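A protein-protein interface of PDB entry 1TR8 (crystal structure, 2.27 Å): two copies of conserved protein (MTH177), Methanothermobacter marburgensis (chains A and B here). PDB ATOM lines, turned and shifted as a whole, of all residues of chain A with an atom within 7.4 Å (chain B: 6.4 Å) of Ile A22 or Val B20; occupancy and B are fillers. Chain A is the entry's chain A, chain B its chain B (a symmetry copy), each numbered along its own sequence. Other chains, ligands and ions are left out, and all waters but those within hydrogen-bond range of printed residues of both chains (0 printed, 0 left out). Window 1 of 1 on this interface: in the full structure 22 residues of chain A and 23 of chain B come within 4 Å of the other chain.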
ATOM      1  N   VAL A  20      16.625  26.795  22.532  1.00  0.00           N
ATOM      2  CA  VAL A  20      17.732  26.974  21.603  1.00  0.00           C
ATOM      3  C   VAL A  20      18.558  25.717  21.727  1.00  0.00           C
ATOM      4  O   VAL A  20      18.779  25.218  22.838  1.00  0.00           O
ATOM      5  CB  VAL A  20      18.586  28.182  21.986  1.00  0.00           C
ATOM      6  CG1 VAL A  20      19.896  28.208  21.191  1.00  0.00           C
ATOM      7  CG2 VAL A  20      17.767  29.445  21.773  1.00  0.00           C
ATOM      8  N   VAL A  21      18.916  25.163  20.573  1.00  0.00           N
ATOM      9  CA  VAL A  21      19.787  24.007  20.505  1.00  0.00           C
ATOM     10  C   VAL A  21      21.021  24.383  19.700  1.00  0.00           C
ATOM     11  O   VAL A  21      20.898  24.819  18.548  1.00  0.00           O
ATOM     12  CB  VAL A  21      19.115  22.812  19.806  1.00  0.00           C
ATOM     13  CG1 VAL A  21      20.091  21.646  19.755  1.00  0.00           C
ATOM     14  CG2 VAL A  21      17.798  22.427  20.506  1.00  0.00           C
ATOM     15  N   ILE A  22      22.187  24.106  20.279  1.00  0.00           N
ATOM     16  CA  ILE A  22      23.466  24.288  19.615  1.00  0.00           C
ATOM     17  C   ILE A  22      24.068  22.923  19.301  1.00  0.00           C
ATOM     18  O   ILE A  22      24.412  22.174  20.210  1.00  0.00           O
ATOM     19  CB  ILE A  22      24.407  25.099  20.494  1.00  0.00           C
ATOM     20  CG1 ILE A  22      23.704  26.373  20.964  1.00  0.00           C
ATOM     21  CG2 ILE A  22      25.625  25.434  19.710  1.00  0.00           C
ATOM     22  CD1 ILE A  22      24.483  27.129  21.979  1.00  0.00           C
ATOM     23  N   LYS A  23      24.287  22.673  18.010  1.00  0.00           N
ATOM     24  CA  LYS A  23      24.619  21.356  17.504  1.00  0.00           C
ATOM     25  C   LYS A  23      26.062  21.299  17.070  1.00  0.00           C
ATOM     26  O   LYS A  23      26.502  22.123  16.273  1.00  0.00           O
ATOM     27  CB  LYS A  23      23.746  21.041  16.293  1.00  0.00           C
ATOM     28  CG  LYS A  23      22.259  20.992  16.611  1.00  0.00           C
ATOM     29  CD  LYS A  23      21.454  20.866  15.335  1.00  0.00           C
ATOM     30  CE  LYS A  23      20.045  20.378  15.603  1.00  0.00           C
ATOM     31  NZ  LYS A  23      19.467  19.802  14.325  1.00  0.00           N
ATOM     32  N   LEU A  24      26.767  20.293  17.570  1.00  0.00           N
ATOM     33  CA  LEU A  24      28.148  20.032  17.205  1.00  0.00           C
ATOM     34  C   LEU A  24      28.165  18.572  16.822  1.00  0.00           C
ATOM     35  O   LEU A  24      27.149  17.920  16.918  1.00  0.00           O
ATOM     36  CB  LEU A  24      29.062  20.303  18.399  1.00  0.00           C
ATOM     37  CG  LEU A  24      29.197  21.750  18.879  1.00  0.00           C
ATOM     38  CD1 LEU A  24      28.192  22.066  19.961  1.00  0.00           C
ATOM     39  CD2 LEU A  24      30.603  22.005  19.412  1.00  0.00           C
ATOM     40  N   LYS A  27      27.861  16.329  20.251  1.00  0.00           N
ATOM     41  CA  LYS A  27      26.927  16.724  21.276  1.00  0.00           C
ATOM     42  C   LYS A  27      26.116  17.914  20.834  1.00  0.00           C
ATOM     43  O   LYS A  27      26.426  18.567  19.844  1.00  0.00           O
ATOM     44  CB  LYS A  27      27.656  17.076  22.581  1.00  0.00           C
ATOM     45  CG  LYS A  27      28.346  18.433  22.584  1.00  0.00           C
ATOM     46  CD  LYS A  27      28.949  18.757  23.945  1.00  0.00           C
ATOM     47  CE  LYS A  27      29.473  20.208  24.022  1.00  0.00           C
ATOM     48  NZ  LYS A  27      30.390  20.436  25.200  1.00  0.00           N
ATOM     49  N   GLU A  28      25.065  18.164  21.607  1.00  0.00           N
ATOM     50  CA  GLU A  28      24.236  19.323  21.469  1.00  0.00           C
ATOM     51  C   GLU A  28      24.032  19.972  22.844  1.00  0.00           C
ATOM     52  O   GLU A  28      24.018  19.305  23.877  1.00  0.00           O
ATOM     53  CB  GLU A  28      22.915  18.905  20.830  1.00  0.00           C
ATOM     54  CG  GLU A  28      23.154  18.065  19.567  1.00  0.00           C
ATOM     55  CD  GLU A  28      21.889  17.668  18.831  1.00  0.00           C
ATOM     56  OE1 GLU A  28      20.835  17.564  19.496  1.00  0.00           O
ATOM     57  OE2 GLU A  28      21.970  17.415  17.598  1.00  0.00           O
ATOM     58  N   ILE A  29      23.910  21.291  22.840  1.00  0.00           N
ATOM     59  CA  ILE A  29      23.701  22.058  24.041  1.00  0.00           C
ATOM     60  C   ILE A  29      22.288  22.594  23.916  1.00  0.00           C
ATOM     61  O   ILE A  29      21.952  23.188  22.911  1.00  0.00           O
ATOM     62  CB  ILE A  29      24.726  23.218  24.157  1.00  0.00           C
ATOM     63  CG1 ILE A  29      26.151  22.666  24.173  1.00  0.00           C
ATOM     64  CG2 ILE A  29      24.456  24.035  25.429  1.00  0.00           C
ATOM     65  CD1 ILE A  29      27.228  23.718  24.126  1.00  0.00           C
ATOM     66  N   ILE A  30      21.463  22.354  24.928  1.00  0.00           N
ATOM     67  CA  ILE A  30      20.071  22.752  24.886  1.00  0.00           C
ATOM     68  C   ILE A  30      19.809  23.757  26.006  1.00  0.00           C
ATOM     69  O   ILE A  30      20.135  23.490  27.173  1.00  0.00           O
ATOM     70  CB  ILE A  30      19.155  21.498  25.071  1.00  0.00           C
ATOM     71  CG1 ILE A  30      19.377  20.492  23.938  1.00  0.00           C
ATOM     72  CG2 ILE A  30      17.682  21.872  25.135  1.00  0.00           C
ATOM     73  CD1 ILE A  30      20.170  19.318  24.389  1.00  0.00           C
ATOM     74  N   ILE A  31      19.255  24.912  25.633  1.00  0.00           N
ATOM     75  CA  ILE A  31      18.816  25.915  26.596  1.00  0.00           C
ATOM     76  C   ILE A  31      17.309  26.089  26.543  1.00  0.00           C
ATOM     77  O   ILE A  31      16.763  26.567  25.543  1.00  0.00           O
ATOM     78  CB  ILE A  31      19.498  27.262  26.314  1.00  0.00           C
ATOM     79  CG1 ILE A  31      21.000  27.047  26.149  1.00  0.00           C
ATOM     80  CG2 ILE A  31      19.225  28.219  27.469  1.00  0.00           C
ATOM     81  CD1 ILE A  31      21.771  28.304  25.863  1.00  0.00           C
ATOM     82  N   TYR A  47      22.921  36.621  17.479  1.00  0.00           N
ATOM     83  CA  TYR A  47      21.968  36.286  18.533  1.00  0.00           C
ATOM     84  C   TYR A  47      22.695  36.102  19.851  1.00  0.00           C
ATOM     85  O   TYR A  47      23.686  35.384  19.888  1.00  0.00           O
ATOM     86  CB  TYR A  47      21.252  34.984  18.202  1.00  0.00           C
ATOM     87  CG  TYR A  47      20.360  35.084  17.005  1.00  0.00           C
ATOM     88  CD1 TYR A  47      19.060  35.558  17.127  1.00  0.00           C
ATOM     89  CD2 TYR A  47      20.812  34.699  15.749  1.00  0.00           C
ATOM     90  CE1 TYR A  47      18.234  35.642  16.020  1.00  0.00           C
ATOM     91  CE2 TYR A  47      20.000  34.793  14.646  1.00  0.00           C
ATOM     92  CZ  TYR A  47      18.708  35.264  14.786  1.00  0.00           C
ATOM     93  OH  TYR A  47      17.910  35.406  13.666  1.00  0.00           O
ATOM     94  N   VAL A  49      21.981  34.662  23.570  1.00  0.00           N
ATOM     95  CA  VAL A  49      21.111  33.639  24.130  1.00  0.00           C
ATOM     96  C   VAL A  49      21.592  33.329  25.525  1.00  0.00           C
ATOM     97  O   VAL A  49      22.689  32.823  25.725  1.00  0.00           O
ATOM     98  CB  VAL A  49      21.175  32.331  23.340  1.00  0.00           C
ATOM     99  CG1 VAL A  49      20.244  31.283  23.958  1.00  0.00           C
ATOM    100  CG2 VAL A  49      20.795  32.570  21.922  1.00  0.00           C
ATOM    101  N   ALA A  53      21.977  25.921  30.641  1.00  0.00           N
ATOM    102  CA  ALA A  53      22.321  25.004  29.576  1.00  0.00           C
ATOM    103  C   ALA A  53      22.387  23.576  30.073  1.00  0.00           C
ATOM    104  O   ALA A  53      22.812  23.325  31.216  1.00  0.00           O
ATOM    105  CB  ALA A  53      23.644  25.399  28.986  1.00  0.00           C
ATOM    106  N   ARG A  54      21.959  22.659  29.204  1.00  0.00           N
ATOM    107  CA  ARG A  54      22.132  21.222  29.395  1.00  0.00           C
ATOM    108  C   ARG A  54      22.755  20.576  28.150  1.00  0.00           C
ATOM    109  O   ARG A  54      22.651  21.103  27.033  1.00  0.00           O
ATOM    110  CB  ARG A  54      20.783  20.556  29.673  1.00  0.00           C
ATOM    111  CG  ARG A  54      20.170  20.910  30.998  1.00  0.00           C
ATOM    112  CD  ARG A  54      18.885  20.108  31.273  1.00  0.00           C
ATOM    113  NE  ARG A  54      18.423  20.271  32.641  1.00  0.00           N
ATOM    114  CZ  ARG A  54      17.673  21.283  33.042  1.00  0.00           C
ATOM    115  NH1 ARG A  54      17.284  22.211  32.174  1.00  0.00           N
ATOM    116  NH2 ARG A  54      17.287  21.367  34.305  1.00  0.00           N
ATOM    117  N   ARG A  56      23.600  17.071  25.739  1.00  0.00           N
ATOM    118  CA  ARG A  56      23.055  15.838  25.164  1.00  0.00           C
ATOM    119  C   ARG A  56      24.101  15.287  24.216  1.00  0.00           C
ATOM    120  O   ARG A  56      24.434  15.947  23.245  1.00  0.00           O
ATOM    121  CB  ARG A  56      21.837  16.233  24.347  1.00  0.00           C
ATOM    122  CG  ARG A  56      21.025  15.109  23.857  1.00  0.00           C
ATOM    123  CD  ARG A  56      19.625  15.575  23.524  1.00  0.00           C
ATOM    124  NE  ARG A  56      19.617  16.478  22.395  1.00  0.00           N
ATOM    125  CZ  ARG A  56      18.571  17.197  22.038  1.00  0.00           C
ATOM    126  NH1 ARG A  56      17.475  17.173  22.785  1.00  0.00           N
ATOM    127  NH2 ARG A  56      18.637  17.966  20.962  1.00  0.00           N
ATOM    128  N   LEU B  14      33.755  28.895  20.498  1.00  0.00           N
ATOM    129  CA  LEU B  14      33.212  27.555  20.479  1.00  0.00           C
ATOM    130  C   LEU B  14      33.346  27.011  19.065  1.00  0.00           C
ATOM    131  O   LEU B  14      32.700  27.491  18.128  1.00  0.00           O
ATOM    132  CB  LEU B  14      31.766  27.541  20.960  1.00  0.00           C
ATOM    133  CG  LEU B  14      31.209  26.144  21.236  1.00  0.00           C
ATOM    134  CD1 LEU B  14      32.047  25.405  22.256  1.00  0.00           C
ATOM    135  CD2 LEU B  14      29.745  26.210  21.698  1.00  0.00           C
ATOM    136  N   VAL B  17      30.794  24.205  15.426  1.00  0.00           N
ATOM    137  CA  VAL B  17      29.348  24.272  15.556  1.00  0.00           C
ATOM    138  C   VAL B  17      28.736  24.162  14.170  1.00  0.00           C
ATOM    139  O   VAL B  17      28.986  24.995  13.311  1.00  0.00           O
ATOM    140  CB  VAL B  17      28.879  25.534  16.278  1.00  0.00           C
ATOM    141  CG1 VAL B  17      27.376  25.537  16.397  1.00  0.00           C
ATOM    142  CG2 VAL B  17      29.478  25.582  17.665  1.00  0.00           C
ATOM    143  N   GLU B  18      27.953  23.109  13.974  1.00  0.00           N
ATOM    144  CA  GLU B  18      27.348  22.796  12.685  1.00  0.00           C
ATOM    145  C   GLU B  18      26.096  23.627  12.473  1.00  0.00           C
ATOM    146  O   GLU B  18      25.739  23.939  11.342  1.00  0.00           O
ATOM    147  CB  GLU B  18      27.009  21.301  12.613  1.00  0.00           C
ATOM    148  CG  GLU B  18      28.219  20.388  12.780  1.00  0.00           C
ATOM    149  CD  GLU B  18      27.906  18.909  12.621  1.00  0.00           C
ATOM    150  OE1 GLU B  18      26.725  18.514  12.700  1.00  0.00           O
ATOM    151  OE2 GLU B  18      28.851  18.123  12.420  1.00  0.00           O
ATOM    152  N   GLU B  19      25.424  24.000  13.554  1.00  0.00           N
ATOM    153  CA  GLU B  19      24.097  24.575  13.416  1.00  0.00           C
ATOM    154  C   GLU B  19      23.534  25.022  14.742  1.00  0.00           C
ATOM    155  O   GLU B  19      23.645  24.333  15.736  1.00  0.00           O
ATOM    156  CB  GLU B  19      23.154  23.508  12.833  1.00  0.00           C
ATOM    157  CG  GLU B  19      21.767  24.017  12.489  1.00  0.00           C
ATOM    158  CD  GLU B  19      20.901  22.945  11.857  1.00  0.00           C
ATOM    159  OE1 GLU B  19      20.373  22.075  12.575  1.00  0.00           O
ATOM    160  OE2 GLU B  19      20.738  22.979  10.621  1.00  0.00           O
ATOM    161  N   VAL B  20      22.895  26.175  14.757  1.00  0.00           N
ATOM    162  CA  VAL B  20      22.115  26.590  15.908  1.00  0.00           C
ATOM    163  C   VAL B  20      20.677  26.717  15.430  1.00  0.00           C
ATOM    164  O   VAL B  20      20.437  27.280  14.381  1.00  0.00           O
ATOM    165  CB  VAL B  20      22.610  27.948  16.460  1.00  0.00           C
ATOM    166  CG1 VAL B  20      21.698  28.467  17.560  1.00  0.00           C
ATOM    167  CG2 VAL B  20      24.005  27.826  16.978  1.00  0.00           C
ATOM    168  N   VAL B  21      19.751  26.164  16.201  1.00  0.00           N
ATOM    169  CA  VAL B  21      18.315  26.221  15.961  1.00  0.00           C
ATOM    170  C   VAL B  21      17.620  26.965  17.117  1.00  0.00           C
ATOM    171  O   VAL B  21      17.813  26.659  18.295  1.00  0.00           O
ATOM    172  CB  VAL B  21      17.706  24.803  15.938  1.00  0.00           C
ATOM    173  CG1 VAL B  21      16.197  24.883  15.742  1.00  0.00           C
ATOM    174  CG2 VAL B  21      18.355  23.918  14.841  1.00  0.00           C
ATOM    175  N   ILE B  22      16.830  27.972  16.774  1.00  0.00           N
ATOM    176  CA  ILE B  22      16.031  28.711  17.749  1.00  0.00           C
ATOM    177  C   ILE B  22      14.571  28.336  17.538  1.00  0.00           C
ATOM    178  O   ILE B  22      14.038  28.534  16.454  1.00  0.00           O
ATOM    179  CB  ILE B  22      16.239  30.216  17.555  1.00  0.00           C
ATOM    180  CG1 ILE B  22      17.730  30.543  17.694  1.00  0.00           C
ATOM    181  CG2 ILE B  22      15.419  31.041  18.564  1.00  0.00           C
ATOM    182  CD1 ILE B  22      18.063  31.918  17.235  1.00  0.00           C
ATOM    183  N   ILE B  29      14.189  29.175  13.780  1.00  0.00           N
ATOM    184  CA  ILE B  29      15.231  29.901  13.055  1.00  0.00           C
ATOM    185  C   ILE B  29      16.495  29.051  13.092  1.00  0.00           C
ATOM    186  O   ILE B  29      16.889  28.615  14.149  1.00  0.00           O
ATOM    187  CB  ILE B  29      15.489  31.316  13.660  1.00  0.00           C
ATOM    188  CG1 ILE B  29      14.222  32.177  13.590  1.00  0.00           C
ATOM    189  CG2 ILE B  29      16.578  32.047  12.871  1.00  0.00           C
ATOM    190  CD1 ILE B  29      14.296  33.444  14.464  1.00  0.00           C
ATOM    191  N   ILE B  30      17.115  28.837  11.937  1.00  0.00           N
ATOM    192  CA  ILE B  30      18.281  27.983  11.801  1.00  0.00           C
ATOM    193  C   ILE B  30      19.410  28.826  11.258  1.00  0.00           C
ATOM    194  O   ILE B  30      19.267  29.498  10.237  1.00  0.00           O
ATOM    195  CB  ILE B  30      18.005  26.816  10.810  1.00  0.00           C
ATOM    196  CG1 ILE B  30      16.852  25.943  11.302  1.00  0.00           C
ATOM    197  CG2 ILE B  30      19.231  25.928  10.619  1.00  0.00           C
ATOM    198  CD1 ILE B  30      15.631  26.163  10.475  1.00  0.00           C
ATOM    199  N   ILE B  31      20.529  28.800  11.967  1.00  0.00           N
ATOM    200  CA  ILE B  31      21.789  29.376  11.510  1.00  0.00           C
ATOM    201  C   ILE B  31      22.808  28.248  11.227  1.00  0.00           C
ATOM    202  O   ILE B  31      23.200  27.519  12.141  1.00  0.00           O
ATOM    203  CB  ILE B  31      22.354  30.345  12.573  1.00  0.00           C
ATOM    204  CG1 ILE B  31      21.318  31.402  12.967  1.00  0.00           C
ATOM    205  CG2 ILE B  31      23.582  31.042  12.016  1.00  0.00           C
ATOM    206  CD1 ILE B  31      20.592  31.156  14.275  1.00  0.00           C
ATOM    207  N   LYS B  32      23.210  28.095   9.972  1.00  0.00           N
ATOM    208  CA  LYS B  32      24.184  27.070   9.574  1.00  0.00           C
ATOM    209  C   LYS B  32      25.645  27.520   9.729  1.00  0.00           C
ATOM    210  O   LYS B  32      25.985  28.670   9.462  1.00  0.00           O
ATOM    211  CB  LYS B  32      23.905  26.637   8.133  1.00  0.00           C
ATOM    212  CG  LYS B  32      22.568  25.893   7.995  1.00  0.00           C
ATOM    213  CD  LYS B  32      22.023  25.951   6.572  1.00  0.00           C
ATOM    214  CE  LYS B  32      20.518  25.660   6.496  1.00  0.00           C
ATOM    215  NZ  LYS B  32      20.041  25.814   5.095  1.00  0.00           N
ATOM    216  N   ASN B  33      26.493  26.603  10.186  1.00  0.00           N
ATOM    217  CA  ASN B  33      27.922  26.871  10.437  1.00  0.00           C
ATOM    218  C   ASN B  33      28.170  28.265  11.013  1.00  0.00           C
ATOM    219  O   ASN B  33      28.848  29.095  10.427  1.00  0.00           O
ATOM    220  CB  ASN B  33      28.741  26.680   9.164  1.00  0.00           C
ATOM    221  CG  ASN B  33      28.625  25.270   8.592  1.00  0.00           C
ATOM    222  OD1 ASN B  33      28.476  25.106   7.377  1.00  0.00           O
ATOM    223  ND2 ASN B  33      28.756  24.253   9.448  1.00  0.00           N
ATOM    224  N   PRO B  34      27.538  28.558  12.130  1.00  0.00           N
ATOM    225  CA  PRO B  34      27.688  29.868  12.734  1.00  0.00           C
ATOM    226  C   PRO B  34      29.056  30.048  13.395  1.00  0.00           C
ATOM    227  O   PRO B  34      29.762  29.086  13.663  1.00  0.00           O
ATOM    228  CB  PRO B  34      26.576  29.881  13.787  1.00  0.00           C
ATOM    229  CG  PRO B  34      26.376  28.450  14.131  1.00  0.00           C
ATOM    230  CD  PRO B  34      26.586  27.704  12.865  1.00  0.00           C
ATOM    231  N   VAL B  36      30.400  31.107  16.963  1.00  0.00           N
ATOM    232  CA  VAL B  36      29.798  31.088  18.293  1.00  0.00           C
ATOM    233  C   VAL B  36      30.826  31.369  19.396  1.00  0.00           C
ATOM    234  O   VAL B  36      31.843  30.700  19.506  1.00  0.00           O
ATOM    235  CB  VAL B  36      29.105  29.731  18.599  1.00  0.00           C
ATOM    236  CG1 VAL B  36      28.406  29.767  19.927  1.00  0.00           C
ATOM    237  CG2 VAL B  36      28.081  29.390  17.578  1.00  0.00           C
ATOM    238  N   TYR B  47      25.482  32.695  25.053  1.00  0.00           N
ATOM    239  CA  TYR B  47      26.047  32.341  23.758  1.00  0.00           C
ATOM    240  C   TYR B  47      25.759  33.429  22.727  1.00  0.00           C
ATOM    241  O   TYR B  47      24.624  33.874  22.582  1.00  0.00           O
ATOM    242  CB  TYR B  47      25.480  31.010  23.257  1.00  0.00           C
ATOM    243  CG  TYR B  47      25.799  29.826  24.135  1.00  0.00           C
ATOM    244  CD1 TYR B  47      26.855  28.967  23.836  1.00  0.00           C
ATOM    245  CD2 TYR B  47      25.041  29.566  25.265  1.00  0.00           C
ATOM    246  CE1 TYR B  47      27.173  27.919  24.669  1.00  0.00           C
ATOM    247  CE2 TYR B  47      25.339  28.497  26.095  1.00  0.00           C
ATOM    248  CZ  TYR B  47      26.396  27.669  25.794  1.00  0.00           C
ATOM    249  OH  TYR B  47      26.665  26.614  26.654  1.00  0.00           O
ATOM    250  N   VAL B  49      25.837  33.996  18.808  1.00  0.00           N
ATOM    251  CA  VAL B  49      25.767  33.166  17.618  1.00  0.00           C
ATOM    252  C   VAL B  49      25.682  34.071  16.414  1.00  0.00           C
ATOM    253  O   VAL B  49      24.755  34.843  16.291  1.00  0.00           O
ATOM    254  CB  VAL B  49      24.506  32.278  17.670  1.00  0.00           C
ATOM    255  CG1 VAL B  49      24.370  31.424  16.398  1.00  0.00           C
ATOM    256  CG2 VAL B  49      24.520  31.429  18.956  1.00  0.00           C
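Ile A22 touches four residues of chain B.
Printed residues of chain A within 4 Å of Val B17: Ile A22 (3.7 Å) and Lys A23 (3.5 Å).
Of chain A, only Val A21 (3.4 Å) and Ile A22 (3.98 Å) come within 4 Å of Val B20.
Printed residues of chain A within 4 Å of Ile B22: Tyr A47 (3.8 Å).
Ile B30 touches none of the printed residues of chain A.
The nearest printed residue of chain A that does not touch Ile B22 is Val A20 (4.2 Å).
Ile A22 touches Val B20, but with the chains exchanged Val A20 does not touch Ile B22 (4.2 Å).
Ile A22 touches Tyr B47, and with the chains exchanged Tyr A47 touches Ile B22.
Ile A29 touches Tyr B47, and with the chains exchanged Tyr A47 touches Ile B29.
Tyr A47 touches Val B49, and with the chains exchanged Val A49 touches Tyr B47.
Positions printed for both chains: 20, 21, 22, 29, 30, 31, 47 and 49.
Of the 20 pairs that touch across the chains among the printed residues, 12 have their exchanged pair printed and touching as well.
The backbone NH (N) of Ile A31 sits at hydrogen-bond distance from the backbone carbonyl oxygen (O) of Val A20.
N of Ile A22 sits at hydrogen-bond distance from O of Ile A29, 2.8 Å away.
The backbone carbonyl oxygen (O) of Glu B18 sits at hydrogen-bond distance from the backbone NH (N) of Asn B33, at 3.0 Å.
The backbone NH (N) of Ile B31 lies within hydrogen-bond range of the backbone carbonyl oxygen (O) of Val B20 (2.9 Å).
N of Ile B22 is in hydrogen-bond range of O of Ile B29, 2.7 Å away.
Val A20 touches Val B21 (CA to O, 3.3 Å).
O of Val A21 touches O of Glu B19 (3.96 Å).
Val B20 touches Val A21 (CA to O, 3.4 Å).
CG2 of Ile A22 touches CG1 of Val B17, at 3.7 Å.
Val B20 touches Ile A22 (CG2 to CG2, 3.98 Å).
CD1 of Ile A22 touches CD1 of Tyr B47 (3.5 Å).
O of Lys A23 touches CG1 of Val B17, 3.5 Å away.
OH of Tyr B47 touches CG2 of Ile A29, at 3.6 Å.
Tyr B47 touches Ile A31 (CD2 to CD1, 3.6 Å).
CD1 of Ile B22 touches CD1 of Tyr A47, at 3.8 Å.
Of the 15 printed residues of chain A, 8 touch a printed residue of chain B.
Printed residues of chain A that touch a printed residue of chain B: Val A20, Val A21, Ile A22, Lys A23, Ile A29, Ile A31, Tyr A47 and Val A49.
Hydrophobic or aromatic side chains of chain A that line the printed part of chain B: Val A20, Ile A22, Ile A29, Ile A31, Tyr A47 and Val A49.
Along chain A the printed residues that touch a printed residue of chain B span positions 20 to 49.
Hydrophobic or aromatic side chains of chain B within 4 Å of the printed part of chain A: Val B17, Val B20, Val B21, Ile B22, Ile B29, Ile B31, Tyr B47 and Val B49.
Among the printed residues, 20 pairs touch across the chains.
Among the printed residues, Asp or Glu carboxylates within 4 Å of a Lys or Arg side-chain nitrogen of the other chain: Lys A23 with Glu B19.
The backbone carbonyl oxygen (O) of Val A21 is in hydrogen-bond range of the backbone NH (N) of Val B21 (2.9 Å).
The backbone carbonyl oxygen (O) of Lys A23 lies within hydrogen-bond range of the backbone NH (N) of Glu B18 (2.9 Å).
The side-chain amino group (NZ) of Lys A23 lies within salt-bridge range of the side-chain carboxylate (OE1) of Glu B19, 3.0 Å away.
O of Tyr A47 sits at hydrogen-bond distance from N of Val B49, 2.8 Å away.
The backbone carbonyl oxygen of Val A49 is in hydrogen-bond range of the backbone NH of Tyr B47 (2.9 Å).
O of Tyr A47 lies close to O of Tyr B47 (3.2 Å).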
